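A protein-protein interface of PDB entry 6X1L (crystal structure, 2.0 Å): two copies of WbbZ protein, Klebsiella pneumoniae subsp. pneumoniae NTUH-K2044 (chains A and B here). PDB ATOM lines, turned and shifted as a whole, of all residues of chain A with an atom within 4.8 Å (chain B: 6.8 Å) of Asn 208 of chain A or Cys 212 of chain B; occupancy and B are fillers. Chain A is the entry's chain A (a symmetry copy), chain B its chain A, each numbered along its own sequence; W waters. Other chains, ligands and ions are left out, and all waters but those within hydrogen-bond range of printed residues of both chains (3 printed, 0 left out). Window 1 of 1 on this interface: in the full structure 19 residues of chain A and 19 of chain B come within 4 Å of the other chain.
The backbone NH (N) of Ser 209 of chain B is in hydrogen-bond range of the side-chain sulfur (SG) of Cys 212 of chain A, at 3.3 Å.
The side-chain sulfur (SG) of Cys 212 of chain B is in hydrogen-bond range of the backbone NH (N) of Ser 209 of chain A (3.3 Å).
The side-chain amide nitrogen (ND2) of Asn 215 of chain B sits close to the backbone carbonyl oxygen (O) of Phe 204 of chain A (3.4 Å).
The side-chain amide nitrogen of Asn 215 of chain B sits close to the backbone NH of Leu 205 of chain A (3.5 Å).
ND2 of Asn 215 of chain B lies close to ND2 of Asn 208 of chain A.
The backbone carbonyl oxygen of Ile 191 of chain B lies within hydrogen-bond range of the side-chain hydroxyl of Thr 194 of chain B (3.0 Å).
The guanidinium group (NH1) of Arg 211 of chain B is in hydrogen-bond range of the side-chain amide oxygen (OD1) of Asn 208 of chain B (2.8 Å).
ND2 of Asn 215 of chain B lies close to O of Arg 211 of chain B.
The backbone carbonyl oxygen (O) of Phe 204 of chain A sits at hydrogen-bond distance from the side-chain amide nitrogen (ND2) of Asn 208 of chain A, 3.2 Å away.
NH1 of Arg 211 of chain A is in hydrogen-bond range of OD1 of Asn 208 of chain A (2.8 Å).
O of Asn 208 of chain A sits at hydrogen-bond distance from SG of Cys 212 of chain A (3.5 Å).
Among the printed residues, pairs that only touch across the chains: Phe 204 of chain A with Ser 161 of chain B, Trp 195 of chain A with Ile 191 of chain B, Trp 195 of chain A with Thr 194 of chain B, Asn 208 of chain A with Cys 212 of chain B, Cys 212 of chain A with Asn 208 of chain B, Asn 208 of chain A with Arg 211 of chain B, Arg 211 of chain A with Asn 208 of chain B, Cys 212 of chain A with Trp 195 of chain B, Trp 195 of chain A with Cys 212 of chain B, Leu 205 of chain A with Cys 212 of chain B, Asn 208 of chain A with Asn 208 of chain B and Trp 195 of chain A with Met 213 of chain B.
Asn 208 of chain A touches just these residues of chain B: Asn 208, Arg 211, Cys 212 and Asn 215.
Printed residues of chain B within 4 Å of Cys 212 of chain A: Trp 195 (3.6 Å), Asn 208 (3.5 Å) and Ser 209 (3.3 Å).
Thr 210 of chain B touches none of the printed residues of chain A.
Cys 212 of chain B touches four residues of chain A.
Printed residues of chain A within 4 Å of Met 213 of chain B: Trp 195 (3.9997 Å).
The nearest residue of chain B that does not touch Asn 208 of chain A is Ser 209 of chain B (5.4 Å).
Of the 16 printed residues of chain B, 10 touch a printed residue of chain A.
Printed residues of chain B that touch a printed residue of chain A: Ser 161, Ile 191, Thr 194, Trp 195, Asn 208, Ser 209, Arg 211, Cys 212, Met 213 and Asn 215.
Hydrophobic or aromatic side chains of chain B that line the printed part of chain A: Ile 191 and Trp 195.
Among the printed residues, no Asp or Glu carboxylate lies within 4 Å of a Lys or Arg side-chain nitrogen of the other chain.
Trp 195 of chain A touches Cys 212 of chain B, and with the chains exchanged Cys 212 of chain A touches Trp 195 of chain B.
Asn 208 of chain A touches its own counterpart, Asn 208 of chain B.
Asn 208 of chain A touches Arg 211 of chain B, and with the chains exchanged Arg 211 of chain A touches Asn 208 of chain B.
Ser 209 of chain A touches Cys 212 of chain B, and with the chains exchanged Cys 212 of chain A touches Ser 209 of chain B.
Of the 17 pairs that touch across the chains among the printed residues, 9 have their exchanged pair printed and touching as well.
Water W3 lies within hydrogen-bond range of the side-chain hydroxyl of Thr 194 of chain B (2.7 Å), the side-chain hydroxyl of Ser 209 of chain B (2.8 Å) and the indole nitrogen of Trp 195 of chain A (3.0 Å).
Water W2 bridges the side-chain hydroxyl (OG) of Ser 209 of chain A and the indole nitrogen (NE1) of Trp 195 of chain B.
Water W1 lies within hydrogen-bond range of O of Tyr 159 of chain B (3.0 Å), ND2 of Asn 208 of chain A (3.1 Å) and OD1 of Asn 215 of chain B (3.2 Å).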
ATOM      1  N   TRP A 195       3.432 -14.170 -26.720  1.00  0.00           N
ATOM      2  CA  TRP A 195       3.293 -14.112 -28.169  1.00  0.00           C
ATOM      3  C   TRP A 195       1.995 -13.386 -28.495  1.00  0.00           C
ATOM      4  O   TRP A 195       0.936 -13.752 -27.980  1.00  0.00           O
ATOM      5  CB  TRP A 195       3.304 -15.516 -28.773  1.00  0.00           C
ATOM      6  CG  TRP A 195       4.675 -16.119 -28.813  1.00  0.00           C
ATOM      7  CD1 TRP A 195       5.301 -16.800 -27.811  1.00  0.00           C
ATOM      8  CD2 TRP A 195       5.594 -16.076 -29.907  1.00  0.00           C
ATOM      9  NE1 TRP A 195       6.559 -17.187 -28.216  1.00  0.00           N
ATOM     10  CE2 TRP A 195       6.761 -16.757 -29.502  1.00  0.00           C
ATOM     11  CE3 TRP A 195       5.544 -15.532 -31.193  1.00  0.00           C
ATOM     12  CZ2 TRP A 195       7.863 -16.905 -30.336  1.00  0.00           C
ATOM     13  CZ3 TRP A 195       6.641 -15.679 -32.021  1.00  0.00           C
ATOM     14  CH2 TRP A 195       7.786 -16.362 -31.590  1.00  0.00           C
ATOM     15  N   PHE A 204       2.263 -25.627 -34.917  1.00  0.00           N
ATOM     16  CA  PHE A 204       3.340 -25.910 -33.973  1.00  0.00           C
ATOM     17  C   PHE A 204       3.559 -24.735 -33.032  1.00  0.00           C
ATOM     18  O   PHE A 204       3.643 -24.909 -31.809  1.00  0.00           O
ATOM     19  CB  PHE A 204       4.620 -26.255 -34.731  1.00  0.00           C
ATOM     20  CG  PHE A 204       4.568 -27.587 -35.419  1.00  0.00           C
ATOM     21  CD1 PHE A 204       4.995 -28.735 -34.765  1.00  0.00           C
ATOM     22  CD2 PHE A 204       4.082 -27.696 -36.712  1.00  0.00           C
ATOM     23  CE1 PHE A 204       4.947 -29.965 -35.394  1.00  0.00           C
ATOM     24  CE2 PHE A 204       4.028 -28.923 -37.348  1.00  0.00           C
ATOM     25  CZ  PHE A 204       4.460 -30.060 -36.688  1.00  0.00           C
ATOM     26  N   LEU A 205       3.625 -23.523 -33.586  1.00  0.00           N
ATOM     27  CA  LEU A 205       3.777 -22.332 -32.761  1.00  0.00           C
ATOM     28  C   LEU A 205       2.606 -22.169 -31.801  1.00  0.00           C
ATOM     29  O   LEU A 205       2.800 -21.795 -30.637  1.00  0.00           O
ATOM     30  CB  LEU A 205       3.937 -21.102 -33.655  1.00  0.00           C
ATOM     31  CG  LEU A 205       4.122 -19.736 -32.995  1.00  0.00           C
ATOM     32  CD1 LEU A 205       5.153 -19.806 -31.876  1.00  0.00           C
ATOM     33  CD2 LEU A 205       4.542 -18.723 -34.045  1.00  0.00           C
ATOM     34  N   ALA A 206       1.379 -22.457 -32.259  1.00  0.00           N
ATOM     35  CA  ALA A 206       0.234 -22.358 -31.360  1.00  0.00           C
ATOM     36  C   ALA A 206       0.338 -23.369 -30.226  1.00  0.00           C
ATOM     37  O   ALA A 206       0.100 -23.037 -29.059  1.00  0.00           O
ATOM     38  CB  ALA A 206      -1.086 -22.550 -32.132  1.00  0.00           C
ATOM     39  N   ARG A 207       0.674 -24.619 -30.547  1.00  0.00           N
ATOM     40  CA  ARG A 207       0.706 -25.642 -29.505  1.00  0.00           C
ATOM     41  C   ARG A 207       1.865 -25.419 -28.535  1.00  0.00           C
ATOM     42  O   ARG A 207       1.718 -25.630 -27.324  1.00  0.00           O
ATOM     43  CB  ARG A 207       0.782 -27.032 -30.134  1.00  0.00           C
ATOM     44  CG  ARG A 207      -0.562 -27.491 -30.726  1.00  0.00           C
ATOM     45  CD  ARG A 207      -0.631 -29.006 -30.806  1.00  0.00           C
ATOM     46  NE  ARG A 207      -1.891 -29.491 -31.368  1.00  0.00           N
ATOM     47  CZ  ARG A 207      -2.055 -29.811 -32.646  1.00  0.00           C
ATOM     48  NH1 ARG A 207      -1.044 -29.688 -33.493  1.00  0.00           N
ATOM     49  NH2 ARG A 207      -3.229 -30.260 -33.080  1.00  0.00           N
ATOM     50  N   ASN A 208       3.017 -24.976 -29.037  1.00  0.00           N
ATOM     51  CA  ASN A 208       4.157 -24.784 -28.140  1.00  0.00           C
ATOM     52  C   ASN A 208       3.996 -23.532 -27.285  1.00  0.00           C
ATOM     53  O   ASN A 208       4.383 -23.534 -26.111  1.00  0.00           O
ATOM     54  CB  ASN A 208       5.452 -24.757 -28.949  1.00  0.00           C
ATOM     55  CG  ASN A 208       5.851 -26.135 -29.424  1.00  0.00           C
ATOM     56  OD1 ASN A 208       5.698 -27.119 -28.703  1.00  0.00           O
ATOM     57  ND2 ASN A 208       6.356 -26.216 -30.644  1.00  0.00           N
ATOM     58  N   SER A 209       3.405 -22.467 -27.835  1.00  0.00           N
ATOM     59  CA  SER A 209       3.041 -21.331 -26.994  1.00  0.00           C
ATOM     60  C   SER A 209       2.065 -21.749 -25.904  1.00  0.00           C
ATOM     61  O   SER A 209       2.155 -21.278 -24.763  1.00  0.00           O
ATOM     62  CB  SER A 209       2.439 -20.211 -27.839  1.00  0.00           C
ATOM     63  OG  SER A 209       1.897 -19.197 -27.005  1.00  0.00           O
ATOM     64  N   THR A 210       1.124 -22.637 -26.235  1.00  0.00           N
ATOM     65  CA  THR A 210       0.171 -23.101 -25.234  1.00  0.00           C
ATOM     66  C   THR A 210       0.857 -23.976 -24.189  1.00  0.00           C
ATOM     67  O   THR A 210       0.505 -23.932 -23.002  1.00  0.00           O
ATOM     68  CB  THR A 210      -0.978 -23.846 -25.921  1.00  0.00           C
ATOM     69  OG1 THR A 210      -1.600 -22.976 -26.877  1.00  0.00           O
ATOM     70  CG2 THR A 210      -2.013 -24.286 -24.916  1.00  0.00           C
ATOM     71  N   ARG A 211       1.841 -24.773 -24.608  1.00  0.00           N
ATOM     72  CA  ARG A 211       2.643 -25.520 -23.642  1.00  0.00           C
ATOM     73  C   ARG A 211       3.328 -24.582 -22.657  1.00  0.00           C
ATOM     74  O   ARG A 211       3.337 -24.842 -21.448  1.00  0.00           O
ATOM     75  CB  ARG A 211       3.671 -26.388 -24.368  1.00  0.00           C
ATOM     76  CG  ARG A 211       3.055 -27.602 -25.043  1.00  0.00           C
ATOM     77  CD  ARG A 211       4.098 -28.555 -25.621  1.00  0.00           C
ATOM     78  NE  ARG A 211       3.448 -29.718 -26.221  1.00  0.00           N
ATOM     79  CZ  ARG A 211       3.189 -29.849 -27.520  1.00  0.00           C
ATOM     80  NH1 ARG A 211       3.544 -28.897 -28.373  1.00  0.00           N
ATOM     81  NH2 ARG A 211       2.579 -30.937 -27.968  1.00  0.00           N
ATOM     82  N   CYS A 212       3.889 -23.475 -23.156  1.00  0.00           N
ATOM     83  CA  CYS A 212       4.539 -22.499 -22.283  1.00  0.00           C
ATOM     84  C   CYS A 212       3.590 -22.014 -21.194  1.00  0.00           C
ATOM     85  O   CYS A 212       3.924 -22.044 -20.005  1.00  0.00           O
ATOM     86  CB  CYS A 212       5.047 -21.316 -23.104  1.00  0.00           C
ATOM     87  SG  CYS A 212       6.508 -21.667 -24.100  1.00  0.00           S
ATOM     88  N   TYR B 159      13.621 -29.961 -31.286  1.00  0.00           N
ATOM     89  CA  TYR B 159      12.899 -28.697 -31.280  1.00  0.00           C
ATOM     90  C   TYR B 159      12.234 -28.380 -32.614  1.00  0.00           C
ATOM     91  O   TYR B 159      11.380 -27.490 -32.664  1.00  0.00           O
ATOM     92  CB  TYR B 159      13.848 -27.546 -30.920  1.00  0.00           C
ATOM     93  CG  TYR B 159      14.526 -27.689 -29.579  1.00  0.00           C
ATOM     94  CD1 TYR B 159      15.708 -28.418 -29.448  1.00  0.00           C
ATOM     95  CD2 TYR B 159      14.002 -27.083 -28.447  1.00  0.00           C
ATOM     96  CE1 TYR B 159      16.331 -28.552 -28.226  1.00  0.00           C
ATOM     97  CE2 TYR B 159      14.625 -27.208 -27.213  1.00  0.00           C
ATOM     98  CZ  TYR B 159      15.791 -27.944 -27.112  1.00  0.00           C
ATOM     99  OH  TYR B 159      16.417 -28.080 -25.892  1.00  0.00           O
ATOM    100  N   SER B 161      10.016 -28.244 -36.006  1.00  0.00           N
ATOM    101  CA  SER B 161       8.692 -28.592 -36.498  1.00  0.00           C
ATOM    102  C   SER B 161       8.730 -29.182 -37.900  1.00  0.00           C
ATOM    103  O   SER B 161       7.775 -29.862 -38.296  1.00  0.00           O
ATOM    104  CB  SER B 161       7.783 -27.359 -36.499  1.00  0.00           C
ATOM    105  OG  SER B 161       8.177 -26.434 -37.501  1.00  0.00           O
ATOM    106  N   ILE B 191      10.966 -11.536 -31.323  1.00  0.00           N
ATOM    107  CA  ILE B 191      10.591 -12.796 -30.686  1.00  0.00           C
ATOM    108  C   ILE B 191      11.396 -13.081 -29.431  1.00  0.00           C
ATOM    109  O   ILE B 191      11.017 -13.959 -28.647  1.00  0.00           O
ATOM    110  CB  ILE B 191      10.735 -13.957 -31.689  1.00  0.00           C
ATOM    111  CG1 ILE B 191      12.173 -14.036 -32.210  1.00  0.00           C
ATOM    112  CG2 ILE B 191       9.744 -13.776 -32.848  1.00  0.00           C
ATOM    113  CD1 ILE B 191      12.455 -15.256 -33.063  1.00  0.00           C
ATOM    114  N   THR B 194       9.359 -12.238 -26.024  1.00  0.00           N
ATOM    115  CA  THR B 194       8.111 -12.946 -25.768  1.00  0.00           C
ATOM    116  C   THR B 194       8.007 -13.322 -24.295  1.00  0.00           C
ATOM    117  O   THR B 194       7.235 -12.717 -23.547  1.00  0.00           O
ATOM    118  CB  THR B 194       8.009 -14.181 -26.665  1.00  0.00           C
ATOM    119  OG1 THR B 194       9.182 -14.993 -26.506  1.00  0.00           O
ATOM    120  CG2 THR B 194       7.886 -13.752 -28.125  1.00  0.00           C
ATOM    121  N   TRP B 195       8.775 -14.316 -23.866  1.00  0.00           N
ATOM    122  CA  TRP B 195       8.926 -14.626 -22.452  1.00  0.00           C
ATOM    123  C   TRP B 195      10.161 -13.902 -21.931  1.00  0.00           C
ATOM    124  O   TRP B 195      11.242 -14.028 -22.512  1.00  0.00           O
ATOM    125  CB  TRP B 195       9.044 -16.135 -22.235  1.00  0.00           C
ATOM    126  CG  TRP B 195       7.731 -16.843 -22.370  1.00  0.00           C
ATOM    127  CD1 TRP B 195       7.153 -17.290 -23.522  1.00  0.00           C
ATOM    128  CD2 TRP B 195       6.825 -17.167 -21.313  1.00  0.00           C
ATOM    129  NE1 TRP B 195       5.939 -17.877 -23.247  1.00  0.00           N
ATOM    130  CE2 TRP B 195       5.716 -17.816 -21.896  1.00  0.00           C
ATOM    131  CE3 TRP B 195       6.842 -16.975 -19.929  1.00  0.00           C
ATOM    132  CZ2 TRP B 195       4.639 -18.272 -21.142  1.00  0.00           C
ATOM    133  CZ3 TRP B 195       5.770 -17.428 -19.181  1.00  0.00           C
ATOM    134  CH2 TRP B 195       4.683 -18.070 -19.789  1.00  0.00           C
ATOM    135  N   ARG B 207      12.468 -25.124 -22.872  1.00  0.00           N
ATOM    136  CA  ARG B 207      12.512 -25.838 -24.145  1.00  0.00           C
ATOM    137  C   ARG B 207      11.328 -25.470 -25.036  1.00  0.00           C
ATOM    138  O   ARG B 207      11.477 -25.344 -26.259  1.00  0.00           O
ATOM    139  CB  ARG B 207      12.564 -27.345 -23.902  1.00  0.00           C
ATOM    140  CG  ARG B 207      13.949 -27.825 -23.435  1.00  0.00           C
ATOM    141  CD  ARG B 207      14.148 -29.297 -23.754  1.00  0.00           C
ATOM    142  NE  ARG B 207      15.452 -29.802 -23.323  1.00  0.00           N
ATOM    143  CZ  ARG B 207      15.659 -30.429 -22.171  1.00  0.00           C
ATOM    144  NH1 ARG B 207      14.649 -30.619 -21.333  1.00  0.00           N
ATOM    145  NH2 ARG B 207      16.871 -30.873 -21.856  1.00  0.00           N
ATOM    146  N   ASN B 208      10.146 -25.274 -24.449  1.00  0.00           N
ATOM    147  CA  ASN B 208       8.985 -24.954 -25.277  1.00  0.00           C
ATOM    148  C   ASN B 208       9.027 -23.513 -25.774  1.00  0.00           C
ATOM    149  O   ASN B 208       8.629 -23.241 -26.912  1.00  0.00           O
ATOM    150  CB  ASN B 208       7.702 -25.250 -24.505  1.00  0.00           C
ATOM    151  CG  ASN B 208       7.427 -26.733 -24.411  1.00  0.00           C
ATOM    152  OD1 ASN B 208       7.657 -27.478 -25.363  1.00  0.00           O
ATOM    153  ND2 ASN B 208       6.947 -27.174 -23.261  1.00  0.00           N
ATOM    154  N   SER B 209       9.530 -22.581 -24.958  1.00  0.00           N
ATOM    155  CA  SER B 209       9.787 -21.238 -25.469  1.00  0.00           C
ATOM    156  C   SER B 209      10.782 -21.271 -26.619  1.00  0.00           C
ATOM    157  O   SER B 209      10.639 -20.528 -27.598  1.00  0.00           O
ATOM    158  CB  SER B 209      10.298 -20.330 -24.354  1.00  0.00           C
ATOM    159  OG  SER B 209      10.741 -19.091 -24.886  1.00  0.00           O
ATOM    160  N   THR B 210      11.799 -22.130 -26.521  1.00  0.00           N
ATOM    161  CA  THR B 210      12.777 -22.233 -27.598  1.00  0.00           C
ATOM    162  C   THR B 210      12.158 -22.860 -28.842  1.00  0.00           C
ATOM    163  O   THR B 210      12.491 -22.477 -29.972  1.00  0.00           O
ATOM    164  CB  THR B 210      13.995 -23.030 -27.115  1.00  0.00           C
ATOM    165  OG1 THR B 210      14.549 -22.389 -25.958  1.00  0.00           O
ATOM    166  CG2 THR B 210      15.051 -23.101 -28.189  1.00  0.00           C
ATOM    167  N   ARG B 211      11.250 -23.821 -28.657  1.00  0.00           N
ATOM    168  CA  ARG B 211      10.504 -24.355 -29.794  1.00  0.00           C
ATOM    169  C   ARG B 211       9.730 -23.255 -30.508  1.00  0.00           C
ATOM    170  O   ARG B 211       9.730 -23.189 -31.743  1.00  0.00           O
ATOM    171  CB  ARG B 211       9.564 -25.468 -29.332  1.00  0.00           C
ATOM    172  CG  ARG B 211      10.289 -26.759 -28.991  1.00  0.00           C
ATOM    173  CD  ARG B 211       9.339 -27.916 -28.694  1.00  0.00           C
ATOM    174  NE  ARG B 211      10.093 -29.135 -28.412  1.00  0.00           N
ATOM    175  CZ  ARG B 211      10.378 -29.577 -27.189  1.00  0.00           C
ATOM    176  NH1 ARG B 211       9.952 -28.916 -26.121  1.00  0.00           N
ATOM    177  NH2 ARG B 211      11.085 -30.689 -27.033  1.00  0.00           N
ATOM    178  N   CYS B 212       9.081 -22.369 -29.743  1.00  0.00           N
ATOM    179  CA  CYS B 212       8.341 -21.258 -30.338  1.00  0.00           C
ATOM    180  C   CYS B 212       9.231 -20.426 -31.252  1.00  0.00           C
ATOM    181  O   CYS B 212       8.887 -20.174 -32.412  1.00  0.00           O
ATOM    182  CB  CYS B 212       7.741 -20.380 -29.242  1.00  0.00           C
ATOM    183  SG  CYS B 212       6.327 -21.103 -28.390  1.00  0.00           S
ATOM    184  N   MET B 213      10.379 -19.987 -30.747  1.00  0.00           N
ATOM    185  CA  MET B 213      11.277 -19.160 -31.544  1.00  0.00           C
ATOM    186  C   MET B 213      11.726 -19.904 -32.794  1.00  0.00           C
ATOM    187  O   MET B 213      11.763 -19.341 -33.888  1.00  0.00           O
ATOM    188  CB  MET B 213      12.502 -18.737 -30.723  1.00  0.00           C
ATOM    189  CG  MET B 213      12.184 -17.898 -29.487  1.00  0.00           C
ATOM    190  SD  MET B 213      13.872 -17.479 -28.554  1.00  0.00           S
ATOM    191  CE  MET B 213      14.505 -16.065 -29.726  1.00  0.00           C
ATOM    192  N   ILE B 214      12.068 -21.181 -32.615  1.00  0.00           N
ATOM    193  CA  ILE B 214      12.498 -22.005 -33.742  1.00  0.00           C
ATOM    194  C   ILE B 214      11.354 -22.204 -34.734  1.00  0.00           C
ATOM    195  O   ILE B 214      11.551 -22.088 -35.950  1.00  0.00           O
ATOM    196  CB  ILE B 214      13.056 -23.347 -33.236  1.00  0.00           C
ATOM    197  CG1 ILE B 214      14.420 -23.134 -32.568  1.00  0.00           C
ATOM    198  CG2 ILE B 214      13.154 -24.358 -34.375  1.00  0.00           C
ATOM    199  CD1 ILE B 214      15.047 -24.402 -32.049  1.00  0.00           C
ATOM    200  N   ASN B 215      10.146 -22.507 -34.236  1.00  0.00           N
ATOM    201  CA  ASN B 215       8.991 -22.641 -35.126  1.00  0.00           C
ATOM    202  C   ASN B 215       8.814 -21.399 -35.984  1.00  0.00           C
ATOM    203  O   ASN B 215       8.539 -21.498 -37.185  1.00  0.00           O
ATOM    204  CB  ASN B 215       7.711 -22.885 -34.326  1.00  0.00           C
ATOM    205  CG  ASN B 215       7.681 -24.237 -33.654  1.00  0.00           C
ATOM    206  OD1 ASN B 215       8.386 -25.166 -34.048  1.00  0.00           O
ATOM    207  ND2 ASN B 215       6.848 -24.356 -32.634  1.00  0.00           N
ATOM    208  N   PHE B 216       8.958 -20.219 -35.376  1.00  0.00           N
ATOM    209  CA  PHE B 216       8.810 -18.975 -36.121  1.00  0.00           C
ATOM    210  C   PHE B 216       9.842 -18.885 -37.235  1.00  0.00           C
ATOM    211  O   PHE B 216       9.510 -18.585 -38.388  1.00  0.00           O
ATOM    212  CB  PHE B 216       8.934 -17.784 -35.170  1.00  0.00           C
ATOM    213  CG  PHE B 216       8.918 -16.454 -35.861  1.00  0.00           C
ATOM    214  CD1 PHE B 216       7.713 -15.854 -36.207  1.00  0.00           C
ATOM    215  CD2 PHE B 216      10.103 -15.803 -36.174  1.00  0.00           C
ATOM    216  CE1 PHE B 216       7.688 -14.630 -36.846  1.00  0.00           C
ATOM    217  CE2 PHE B 216      10.085 -14.576 -36.819  1.00  0.00           C
ATOM    218  CZ  PHE B 216       8.875 -13.990 -37.153  1.00  0.00           C
ATOM    219  N   LEU B 217      11.107 -19.165 -36.908  1.00  0.00           N
ATOM    220  CA  LEU B 217      12.190 -18.948 -37.858  1.00  0.00           C
ATOM    221  C   LEU B 217      12.201 -19.986 -38.971  1.00  0.00           C
ATOM    222  O   LEU B 217      12.629 -19.680 -40.089  1.00  0.00           O
ATOM    223  CB  LEU B 217      13.531 -18.959 -37.119  1.00  0.00           C
ATOM    224  CG  LEU B 217      13.719 -17.849 -36.087  1.00  0.00           C
ATOM    225  CD1 LEU B 217      14.933 -18.140 -35.214  1.00  0.00           C
ATOM    226  CD2 LEU B 217      13.867 -16.506 -36.788  1.00  0.00           C
HETATM  227  O   HOH W   1       8.401 -27.865 -32.357  1.00  0.00           O
HETATM  228  O   HOH W   2       3.397 -18.239 -24.787  1.00  0.00           O
HETATM  229  O   HOH W   3       9.140 -17.719 -26.795  1.00  0.00           O
